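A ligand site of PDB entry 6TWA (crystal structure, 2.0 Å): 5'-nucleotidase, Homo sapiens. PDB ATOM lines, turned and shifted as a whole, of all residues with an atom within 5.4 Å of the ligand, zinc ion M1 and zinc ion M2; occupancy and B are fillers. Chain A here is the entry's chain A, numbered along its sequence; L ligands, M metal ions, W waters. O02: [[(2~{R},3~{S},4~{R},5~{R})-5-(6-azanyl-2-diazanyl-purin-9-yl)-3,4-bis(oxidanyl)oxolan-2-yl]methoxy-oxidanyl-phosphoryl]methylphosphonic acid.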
ATOM      1  N   ASP A  11     -17.421   0.766 -31.986  1.00  0.00           N
ATOM      2  CA  ASP A  11     -17.472   1.628 -30.808  1.00  0.00           C
ATOM      3  C   ASP A  11     -18.909   1.895 -30.348  1.00  0.00           C
ATOM      4  O   ASP A  11     -19.269   3.023 -30.056  1.00  0.00           O
ATOM      5  CB  ASP A  11     -16.667   2.913 -31.092  1.00  0.00           C
ATOM      6  CG  ASP A  11     -15.193   2.637 -31.380  1.00  0.00           C
ATOM      7  OD1 ASP A  11     -14.860   2.332 -32.555  1.00  0.00           O
ATOM      8  OD2 ASP A  11     -14.389   2.727 -30.457  1.00  0.00           O
ATOM      9  N   HIS A  13     -20.258   0.700 -27.677  1.00  0.00           N
ATOM     10  CA  HIS A  13     -20.100   1.034 -26.257  1.00  0.00           C
ATOM     11  C   HIS A  13     -21.403   0.968 -25.452  1.00  0.00           C
ATOM     12  O   HIS A  13     -21.833   1.947 -24.806  1.00  0.00           O
ATOM     13  CB  HIS A  13     -19.419   2.422 -26.143  1.00  0.00           C
ATOM     14  CG  HIS A  13     -17.958   2.379 -26.432  1.00  0.00           C
ATOM     15  ND1 HIS A  13     -17.090   1.593 -25.705  1.00  0.00           N
ATOM     16  CD2 HIS A  13     -17.247   3.083 -27.343  1.00  0.00           C
ATOM     17  CE1 HIS A  13     -15.889   1.805 -26.201  1.00  0.00           C
ATOM     18  NE2 HIS A  13     -15.918   2.708 -27.174  1.00  0.00           N
ATOM     19  N   ASP A  60     -15.172  -2.652 -29.560  1.00  0.00           N
ATOM     20  CA  ASP A  60     -15.633  -1.733 -28.527  1.00  0.00           C
ATOM     21  C   ASP A  60     -17.144  -1.702 -28.374  1.00  0.00           C
ATOM     22  O   ASP A  60     -17.762  -0.637 -28.259  1.00  0.00           O
ATOM     23  CB  ASP A  60     -15.047  -0.343 -28.724  1.00  0.00           C
ATOM     24  CG  ASP A  60     -13.702  -0.139 -28.097  1.00  0.00           C
ATOM     25  OD1 ASP A  60     -13.096  -1.142 -27.637  1.00  0.00           O
ATOM     26  OD2 ASP A  60     -13.220   0.995 -28.097  1.00  0.00           O
ATOM     27  N   GLY A  91     -11.825  -5.350 -29.710  1.00  0.00           N
ATOM     28  CA  GLY A  91     -11.383  -3.981 -29.428  1.00  0.00           C
ATOM     29  C   GLY A  91     -10.666  -3.937 -28.109  1.00  0.00           C
ATOM     30  O   GLY A  91     -10.574  -4.943 -27.410  1.00  0.00           O
ATOM     31  N   ASN A  92     -10.179  -2.762 -27.730  1.00  0.00           N
ATOM     32  CA  ASN A  92      -9.462  -2.625 -26.459  1.00  0.00           C
ATOM     33  C   ASN A  92     -10.394  -2.736 -25.276  1.00  0.00           C
ATOM     34  O   ASN A  92     -10.062  -3.447 -24.326  1.00  0.00           O
ATOM     35  CB  ASN A  92      -8.640  -1.336 -26.384  1.00  0.00           C
ATOM     36  CG  ASN A  92      -9.378  -0.070 -26.686  1.00  0.00           C
ATOM     37  OD1 ASN A  92      -9.847   0.122 -27.796  1.00  0.00           O
ATOM     38  ND2 ASN A  92      -9.466   0.845 -25.736  1.00  0.00           N
ATOM     39  N   HIS A  93     -11.614  -2.152 -25.356  1.00  0.00           N
ATOM     40  CA  HIS A  93     -12.570  -2.252 -24.250  1.00  0.00           C
ATOM     41  C   HIS A  93     -13.120  -3.664 -24.023  1.00  0.00           C
ATOM     42  O   HIS A  93     -13.624  -3.912 -22.943  1.00  0.00           O
ATOM     43  CB  HIS A  93     -13.714  -1.254 -24.381  1.00  0.00           C
ATOM     44  CG  HIS A  93     -13.232   0.155 -24.171  1.00  0.00           C
ATOM     45  ND1 HIS A  93     -13.382   0.795 -22.973  1.00  0.00           N
ATOM     46  CD2 HIS A  93     -12.496   0.927 -24.984  1.00  0.00           C
ATOM     47  CE1 HIS A  93     -12.820   1.977 -23.132  1.00  0.00           C
ATOM     48  NE2 HIS A  93     -12.282   2.102 -24.322  1.00  0.00           N
ATOM     49  N   LEU A 159      -4.294   0.869 -22.337  1.00  0.00           N
ATOM     50  CA  LEU A 159      -5.665   1.368 -22.226  1.00  0.00           C
ATOM     51  C   LEU A 159      -6.599   0.478 -21.422  1.00  0.00           C
ATOM     52  O   LEU A 159      -7.566   0.990 -20.868  1.00  0.00           O
ATOM     53  CB  LEU A 159      -6.261   1.476 -23.656  1.00  0.00           C
ATOM     54  CG  LEU A 159      -5.680   2.542 -24.576  1.00  0.00           C
ATOM     55  CD1 LEU A 159      -6.059   2.236 -26.044  1.00  0.00           C
ATOM     56  CD2 LEU A 159      -6.155   3.975 -24.168  1.00  0.00           C
ATOM     57  N   HIS A 195      -9.645  -2.993 -34.910  1.00  0.00           N
ATOM     58  CA  HIS A 195      -9.800  -1.921 -33.963  1.00  0.00           C
ATOM     59  C   HIS A 195      -8.473  -1.261 -33.580  1.00  0.00           C
ATOM     60  O   HIS A 195      -7.962  -1.492 -32.481  1.00  0.00           O
ATOM     61  CB  HIS A 195     -10.492  -2.514 -32.728  1.00  0.00           C
ATOM     62  CG  HIS A 195     -11.086  -1.463 -31.845  1.00  0.00           C
ATOM     63  ND1 HIS A 195     -12.303  -0.906 -32.124  1.00  0.00           N
ATOM     64  CD2 HIS A 195     -10.535  -0.832 -30.791  1.00  0.00           C
ATOM     65  CE1 HIS A 195     -12.501  -0.003 -31.188  1.00  0.00           C
ATOM     66  NE2 HIS A 195     -11.464   0.081 -30.366  1.00  0.00           N
ATOM     67  N   HIS A 218     -12.260   2.484 -33.298  1.00  0.00           N
ATOM     68  CA  HIS A 218     -11.382   3.017 -32.257  1.00  0.00           C
ATOM     69  C   HIS A 218     -11.291   4.556 -32.225  1.00  0.00           C
ATOM     70  O   HIS A 218     -11.442   5.132 -31.147  1.00  0.00           O
ATOM     71  CB  HIS A 218      -9.975   2.399 -32.327  1.00  0.00           C
ATOM     72  CG  HIS A 218      -9.131   2.682 -31.135  1.00  0.00           C
ATOM     73  ND1 HIS A 218      -9.487   2.267 -29.873  1.00  0.00           N
ATOM     74  CD2 HIS A 218      -7.985   3.397 -31.044  1.00  0.00           C
ATOM     75  CE1 HIS A 218      -8.546   2.719 -29.072  1.00  0.00           C
ATOM     76  NE2 HIS A 218      -7.631   3.422 -29.733  1.00  0.00           N
ATOM     77  N   SER A 219     -11.063   5.203 -33.383  1.00  0.00           N
ATOM     78  CA  SER A 219     -10.926   6.654 -33.499  1.00  0.00           C
ATOM     79  C   SER A 219     -12.285   7.363 -33.692  1.00  0.00           C
ATOM     80  O   SER A 219     -12.326   8.587 -33.783  1.00  0.00           O
ATOM     81  CB  SER A 219      -9.976   6.995 -34.641  1.00  0.00           C
ATOM     82  OG  SER A 219     -10.276   6.209 -35.781  1.00  0.00           O
ATOM     83  N   ASN A 220     -13.414   6.600 -33.712  1.00  0.00           N
ATOM     84  CA  ASN A 220     -14.766   7.150 -33.878  1.00  0.00           C
ATOM     85  C   ASN A 220     -14.839   8.009 -35.139  1.00  0.00           C
ATOM     86  O   ASN A 220     -15.555   8.999 -35.162  1.00  0.00           O
ATOM     87  CB  ASN A 220     -15.209   7.962 -32.617  1.00  0.00           C
ATOM     88  CG  ASN A 220     -15.368   7.102 -31.389  1.00  0.00           C
ATOM     89  OD1 ASN A 220     -15.146   5.891 -31.397  1.00  0.00           O
ATOM     90  ND2 ASN A 220     -15.835   7.689 -30.299  1.00  0.00           N
ATOM     91  N   ARG A 329     -12.405  17.191 -25.347  1.00  0.00           N
ATOM     92  CA  ARG A 329     -11.051  16.914 -25.826  1.00  0.00           C
ATOM     93  C   ARG A 329     -10.449  18.114 -26.515  1.00  0.00           C
ATOM     94  O   ARG A 329      -9.308  18.047 -26.954  1.00  0.00           O
ATOM     95  CB  ARG A 329     -11.034  15.688 -26.742  1.00  0.00           C
ATOM     96  CG  ARG A 329     -11.545  14.463 -26.043  1.00  0.00           C
ATOM     97  CD  ARG A 329     -11.368  13.218 -26.896  1.00  0.00           C
ATOM     98  NE  ARG A 329     -11.976  12.057 -26.259  1.00  0.00           N
ATOM     99  CZ  ARG A 329     -11.754  10.790 -26.590  1.00  0.00           C
ATOM    100  NH1 ARG A 329     -10.895  10.490 -27.572  1.00  0.00           N
ATOM    101  NH2 ARG A 329     -12.378   9.809 -25.957  1.00  0.00           N
ATOM    102  N   LEU A 364      -7.905  16.130 -14.938  1.00  0.00           N
ATOM    103  CA  LEU A 364      -8.765  15.026 -15.384  1.00  0.00           C
ATOM    104  C   LEU A 364      -8.643  14.901 -16.898  1.00  0.00           C
ATOM    105  O   LEU A 364      -8.916  15.862 -17.607  1.00  0.00           O
ATOM    106  CB  LEU A 364     -10.227  15.376 -14.987  1.00  0.00           C
ATOM    107  CG  LEU A 364     -11.390  14.639 -15.644  1.00  0.00           C
ATOM    108  CD1 LEU A 364     -11.307  13.137 -15.388  1.00  0.00           C
ATOM    109  CD2 LEU A 364     -12.720  15.200 -15.150  1.00  0.00           C
ATOM    110  N   ASN A 365      -8.259  13.711 -17.400  1.00  0.00           N
ATOM    111  CA  ASN A 365      -8.176  13.474 -18.855  1.00  0.00           C
ATOM    112  C   ASN A 365      -9.586  13.582 -19.509  1.00  0.00           C
ATOM    113  O   ASN A 365     -10.554  12.978 -19.034  1.00  0.00           O
ATOM    114  CB  ASN A 365      -7.512  12.091 -19.144  1.00  0.00           C
ATOM    115  CG  ASN A 365      -8.220  10.870 -18.587  1.00  0.00           C
ATOM    116  OD1 ASN A 365      -8.380  10.730 -17.357  1.00  0.00           O
ATOM    117  ND2 ASN A 365      -8.655   9.936 -19.449  1.00  0.00           N
ATOM    118  N   GLY A 366      -9.700  14.360 -20.573  1.00  0.00           N
ATOM    119  CA  GLY A 366     -10.962  14.522 -21.304  1.00  0.00           C
ATOM    120  C   GLY A 366     -11.547  13.220 -21.867  1.00  0.00           C
ATOM    121  O   GLY A 366     -12.773  13.065 -21.957  1.00  0.00           O
ATOM    122  N   GLY A 367     -10.674  12.258 -22.192  1.00  0.00           N
ATOM    123  CA  GLY A 367     -11.119  10.956 -22.708  1.00  0.00           C
ATOM    124  C   GLY A 367     -11.782  10.078 -21.649  1.00  0.00           C
ATOM    125  O   GLY A 367     -12.403   9.071 -22.002  1.00  0.00           O
ATOM    126  N   GLY A 368     -11.608  10.413 -20.358  1.00  0.00           N
ATOM    127  CA  GLY A 368     -12.257   9.742 -19.250  1.00  0.00           C
ATOM    128  C   GLY A 368     -13.723  10.126 -19.068  1.00  0.00           C
ATOM    129  O   GLY A 368     -14.426   9.453 -18.315  1.00  0.00           O
ATOM    130  N   ARG A 370     -17.027   9.958 -20.573  1.00  0.00           N
ATOM    131  CA  ARG A 370     -17.510   9.090 -21.646  1.00  0.00           C
ATOM    132  C   ARG A 370     -18.897   9.461 -22.195  1.00  0.00           C
ATOM    133  O   ARG A 370     -19.311   8.888 -23.202  1.00  0.00           O
ATOM    134  CB  ARG A 370     -17.457   7.622 -21.179  1.00  0.00           C
ATOM    135  CG  ARG A 370     -16.077   7.149 -20.727  1.00  0.00           C
ATOM    136  CD  ARG A 370     -15.007   7.136 -21.797  1.00  0.00           C
ATOM    137  NE  ARG A 370     -15.277   6.097 -22.794  1.00  0.00           N
ATOM    138  CZ  ARG A 370     -14.524   5.836 -23.853  1.00  0.00           C
ATOM    139  NH1 ARG A 370     -14.869   4.876 -24.704  1.00  0.00           N
ATOM    140  NH2 ARG A 370     -13.413   6.529 -24.072  1.00  0.00           N
ATOM    141  N   PHE A 392     -15.648   3.313 -15.778  1.00  0.00           N
ATOM    142  CA  PHE A 392     -14.495   2.452 -15.502  1.00  0.00           C
ATOM    143  C   PHE A 392     -14.329   1.919 -14.095  1.00  0.00           C
ATOM    144  O   PHE A 392     -13.564   0.964 -13.932  1.00  0.00           O
ATOM    145  CB  PHE A 392     -13.187   3.163 -15.881  1.00  0.00           C
ATOM    146  CG  PHE A 392     -13.159   3.553 -17.334  1.00  0.00           C
ATOM    147  CD1 PHE A 392     -13.201   2.599 -18.323  1.00  0.00           C
ATOM    148  CD2 PHE A 392     -13.236   4.882 -17.703  1.00  0.00           C
ATOM    149  CE1 PHE A 392     -13.255   2.952 -19.657  1.00  0.00           C
ATOM    150  CE2 PHE A 392     -13.247   5.244 -19.039  1.00  0.00           C
ATOM    151  CZ  PHE A 392     -13.290   4.281 -20.005  1.00  0.00           C
ATOM    152  N   SER A 420      -8.622  14.949 -31.421  1.00  0.00           N
ATOM    153  CA  SER A 420      -9.663  14.378 -30.532  1.00  0.00           C
ATOM    154  C   SER A 420      -9.105  13.227 -29.681  1.00  0.00           C
ATOM    155  O   SER A 420      -9.745  12.192 -29.512  1.00  0.00           O
ATOM    156  CB  SER A 420     -10.891  13.921 -31.324  1.00  0.00           C
ATOM    157  OG  SER A 420     -12.033  13.718 -30.509  1.00  0.00           O
ATOM    158  N   THR A 421      -7.900  13.433 -29.131  1.00  0.00           N
ATOM    159  CA  THR A 421      -7.232  12.456 -28.271  1.00  0.00           C
ATOM    160  C   THR A 421      -7.633  12.744 -26.802  1.00  0.00           C
ATOM    161  O   THR A 421      -7.950  13.892 -26.437  1.00  0.00           O
ATOM    162  CB  THR A 421      -5.741  12.430 -28.581  1.00  0.00           C
ATOM    163  OG1 THR A 421      -5.202  13.746 -28.403  1.00  0.00           O
ATOM    164  CG2 THR A 421      -5.443  11.952 -30.004  1.00  0.00           C
ATOM    165  N   GLY A 422      -7.693  11.685 -26.014  1.00  0.00           N
ATOM    166  CA  GLY A 422      -8.183  11.772 -24.643  1.00  0.00           C
ATOM    167  C   GLY A 422      -7.339  12.494 -23.612  1.00  0.00           C
ATOM    168  O   GLY A 422      -7.871  12.820 -22.552  1.00  0.00           O
ATOM    169  N   GLU A 423      -6.047  12.771 -23.904  1.00  0.00           N
ATOM    170  CA  GLU A 423      -5.141  13.450 -22.967  1.00  0.00           C
ATOM    171  C   GLU A 423      -5.412  14.938 -22.744  1.00  0.00           C
ATOM    172  O   GLU A 423      -4.756  15.510 -21.887  1.00  0.00           O
ATOM    173  CB  GLU A 423      -3.645  13.241 -23.338  1.00  0.00           C
ATOM    174  CG  GLU A 423      -3.124  13.967 -24.564  1.00  0.00           C
ATOM    175  CD  GLU A 423      -3.368  13.294 -25.892  1.00  0.00           C
ATOM    176  OE1 GLU A 423      -2.857  13.808 -26.910  1.00  0.00           O
ATOM    177  OE2 GLU A 423      -4.040  12.241 -25.912  1.00  0.00           O
ATOM    178  N   PRO A 473      -7.400  11.019 -11.668  1.00  0.00           N
ATOM    179  CA  PRO A 473      -7.742   9.598 -11.760  1.00  0.00           C
ATOM    180  C   PRO A 473      -6.517   8.691 -11.605  1.00  0.00           C
ATOM    181  O   PRO A 473      -5.425   9.091 -11.985  1.00  0.00           O
ATOM    182  CB  PRO A 473      -8.344   9.474 -13.174  1.00  0.00           C
ATOM    183  CG  PRO A 473      -8.698  10.844 -13.581  1.00  0.00           C
ATOM    184  CD  PRO A 473      -7.729  11.743 -12.911  1.00  0.00           C
ATOM    185  N   PHE A 475      -5.813   6.227 -13.419  1.00  0.00           N
ATOM    186  CA  PHE A 475      -5.387   6.088 -14.798  1.00  0.00           C
ATOM    187  C   PHE A 475      -4.236   7.066 -15.133  1.00  0.00           C
ATOM    188  O   PHE A 475      -3.256   6.647 -15.738  1.00  0.00           O
ATOM    189  CB  PHE A 475      -6.600   6.326 -15.723  1.00  0.00           C
ATOM    190  CG  PHE A 475      -6.317   6.265 -17.212  1.00  0.00           C
ATOM    191  CD1 PHE A 475      -6.038   5.060 -17.839  1.00  0.00           C
ATOM    192  CD2 PHE A 475      -6.340   7.424 -17.987  1.00  0.00           C
ATOM    193  CE1 PHE A 475      -5.765   5.003 -19.204  1.00  0.00           C
ATOM    194  CE2 PHE A 475      -6.090   7.365 -19.360  1.00  0.00           C
ATOM    195  CZ  PHE A 475      -5.818   6.146 -19.957  1.00  0.00           C
ATOM    196  N   ASP A 481      -2.551   7.482 -20.907  1.00  0.00           N
ATOM    197  CA  ASP A 481      -2.630   8.535 -21.907  1.00  0.00           C
ATOM    198  C   ASP A 481      -1.309   9.248 -22.192  1.00  0.00           C
ATOM    199  O   ASP A 481      -1.320  10.412 -22.566  1.00  0.00           O
ATOM    200  CB  ASP A 481      -3.738   9.557 -21.518  1.00  0.00           C
ATOM    201  CG  ASP A 481      -5.039   9.452 -22.292  1.00  0.00           C
ATOM    202  OD1 ASP A 481      -5.050   8.785 -23.340  1.00  0.00           O
ATOM    203  OD2 ASP A 481      -6.017  10.068 -21.866  1.00  0.00           O
HETATM  204  PB  O02 L   1     -11.753   3.964 -27.008  1.00  0.00           P
HETATM  205  O1B O02 L   1     -13.167   3.890 -27.456  1.00  0.00           O
HETATM  206  O2B O02 L   1     -10.944   2.647 -27.075  1.00  0.00           O
HETATM  207  O3B O02 L   1     -11.722   4.429 -25.540  1.00  0.00           O
HETATM  208  PA  O02 L   1     -11.515   6.843 -27.729  1.00  0.00           P
HETATM  209  O1A O02 L   1     -12.979   7.149 -27.936  1.00  0.00           O
HETATM  210  O2A O02 L   1     -10.661   7.784 -28.655  1.00  0.00           O
HETATM  211  C3A O02 L   1     -10.889   5.179 -27.992  1.00  0.00           C
HETATM  212  O5' O02 L   1     -11.118   7.023 -26.211  1.00  0.00           O
HETATM  213  C5' O02 L   1      -9.788   6.839 -25.680  1.00  0.00           C
HETATM  214  C4' O02 L   1      -9.590   7.630 -24.402  1.00  0.00           C
HETATM  215  O4' O02 L   1     -10.368   7.079 -23.321  1.00  0.00           O
HETATM  216  C3' O02 L   1      -8.159   7.626 -23.895  1.00  0.00           C
HETATM  217  O3' O02 L   1      -7.418   8.642 -24.553  1.00  0.00           O
HETATM  218  C2' O02 L   1      -8.335   7.902 -22.394  1.00  0.00           C
HETATM  219  O2' O02 L   1      -8.441   9.279 -22.103  1.00  0.00           O
HETATM  220  C1' O02 L   1      -9.681   7.226 -22.084  1.00  0.00           C
HETATM  221  N9  O02 L   1      -9.584   5.944 -21.397  1.00  0.00           N
HETATM  222  C8  O02 L   1      -9.503   4.699 -21.982  1.00  0.00           C
HETATM  223  N7  O02 L   1      -9.473   3.715 -21.127  1.00  0.00           N
HETATM  224  C5  O02 L   1      -9.527   4.340 -19.886  1.00  0.00           C
HETATM  225  C6  O02 L   1      -9.557   3.848 -18.573  1.00  0.00           C
HETATM  226  N6  O02 L   1      -9.499   2.541 -18.250  1.00  0.00           N
HETATM  227  N1  O02 L   1      -9.648   4.726 -17.545  1.00  0.00           N
HETATM  228  C2  O02 L   1      -9.705   6.046 -17.824  1.00  0.00           C
HETATM  229  N3  O02 L   1      -9.692   6.630 -19.056  1.00  0.00           N
HETATM  230  C4  O02 L   1      -9.603   5.717 -20.035  1.00  0.00           C
HETATM  231  N4  O02 L   1      -9.824   6.852 -16.708  1.00  0.00           N
HETATM  232  N5  O02 L   1      -9.911   8.261 -16.662  1.00  0.00           N
HETATM  233 ZN    ZN M   1     -14.431   2.960 -28.471  1.00  0.00          ZN
HETATM  234 ZN    ZN M   2     -11.043   1.382 -28.792  1.00  0.00          ZN
HETATM  235  O   HOH W   1     -11.867   9.424 -14.421  1.00  0.00           O
HETATM  236  O   HOH W   2     -15.191   4.822 -28.928  1.00  0.00           O
HETATM  237  O   HOH W   3     -11.157   9.517 -30.953  1.00  0.00           O
HETATM  238  O   HOH W   4      -7.048   9.112 -27.107  1.00  0.00           O
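Water W2 bridges OD1 of Asn 220 (2.7 Å) and O1A of the ligand (3.4 Å).
Water W4 lies within hydrogen-bond range of an oxygen (O3') of the ligand (2.6 Å) and the backbone NH of Gly 422 (2.9 Å).
Water W3 lies within hydrogen-bond range of an oxygen (O2A) of the ligand (2.9 Å), the backbone carbonyl oxygen (O) of Ser 219 (3.2 Å) and the backbone carbonyl oxygen (O) of Ser 420 (3.4 Å).
Zinc ion M1 is bound by an oxygen (O1B) of the ligand (1.9 Å).
NE2 of His 13 binds zinc ion M1.
Zinc ion M1 is bound by OD2 of Asp 11, at 2.0 Å.
Water W2 binds zinc ion M1 (2.1 Å).
Zinc ion M1 is bound by OD2 of Asp 60.
N of His 93 sits at hydrogen-bond distance from OD1 of Asp 60, at 2.9 Å.
N of Gly 366 is in hydrogen-bond range of O of Gly 422 (3.1 Å).
The side-chain amide nitrogen (ND2) of Asn 92 sits close to a ring nitrogen (NE2) of His 93.
N of Glu 423 lies within hydrogen-bond range of OD2 of Asp 481 (3.4 Å).
NH1 of Arg 329 sits at hydrogen-bond distance from O of Ser 420 (2.8 Å).
The side-chain carboxylate (OD2) of Asp 11 sits close to the side-chain amide oxygen (OD1) of Asn 220 (3.4 Å).
O of Gly 367 lies close to NH2 of Arg 370 (3.4 Å).
A ring nitrogen (NE2) of His 13 sits close to the guanidinium group (NH1) of Arg 370 (3.4 Å).
The backbone carbonyl oxygen (O) of Leu 159 lies close to a nitrogen (N7) of the ligand (3.3 Å).
O of Gly 367 sits close to O4' of the ligand, 3.1 Å away.
Asn 220 touches the ligand (ND2 to O1A, 3.7 Å).
N of Gly 368 touches O2' of the ligand, 3.8 Å away.
Phe 392 touches the ligand.
Phe 475 touches the ligand (CB to N4, 3.4 Å).
17 residues have an atom within 4 Å of the ligand: Asp 11, His 13, Asp 60, Asn 92, His 93, Leu 159, His 218, Asn 220, Arg 329, Asn 365, Gly 367, Gly 368, Arg 370, Phe 392, Gly 422, Phe 475 and Asp 481.
Of the 26 residues printed, 3 come within 4 Å of zinc ion M1.
The guanidinium group of Arg 370 is in salt-bridge range of an oxygen (O3B) of the ligand (3.1 Å).
A ring nitrogen (NE2) of His 93 sits at hydrogen-bond distance from an oxygen (O3B) of the ligand, at 2.7 Å.
An oxygen (O3') of the ligand lies close to the backbone NH (N) of Gly 422, 3.4 Å away.
The guanidinium group (NH1) of Arg 329 lies within salt-bridge range of an oxygen (O2A) of the ligand (2.9 Å).
An oxygen (O2') of the ligand sits at hydrogen-bond distance from the side-chain amide nitrogen (ND2) of Asn 365 (2.7 Å).
The side-chain carboxylate of Asp 481 is in hydrogen-bond range of an oxygen (O2') of the ligand (2.6 Å).
Zinc ion M2 is bound by OD1 of Asn 92 (2.0 Å), NE2 of His 195 (2.1 Å), ND1 of His 218 (2.1 Å), O2B of the ligand (2.1 Å) and OD2 of Asp 60 (2.3 Å).
Within 4 Å of zinc ion M2: Asp 11, Asp 60, Asn 92, His 195 and His 218.
The nearest printed residue that does not touch zinc ion M2 is His 93 (4.1 Å).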
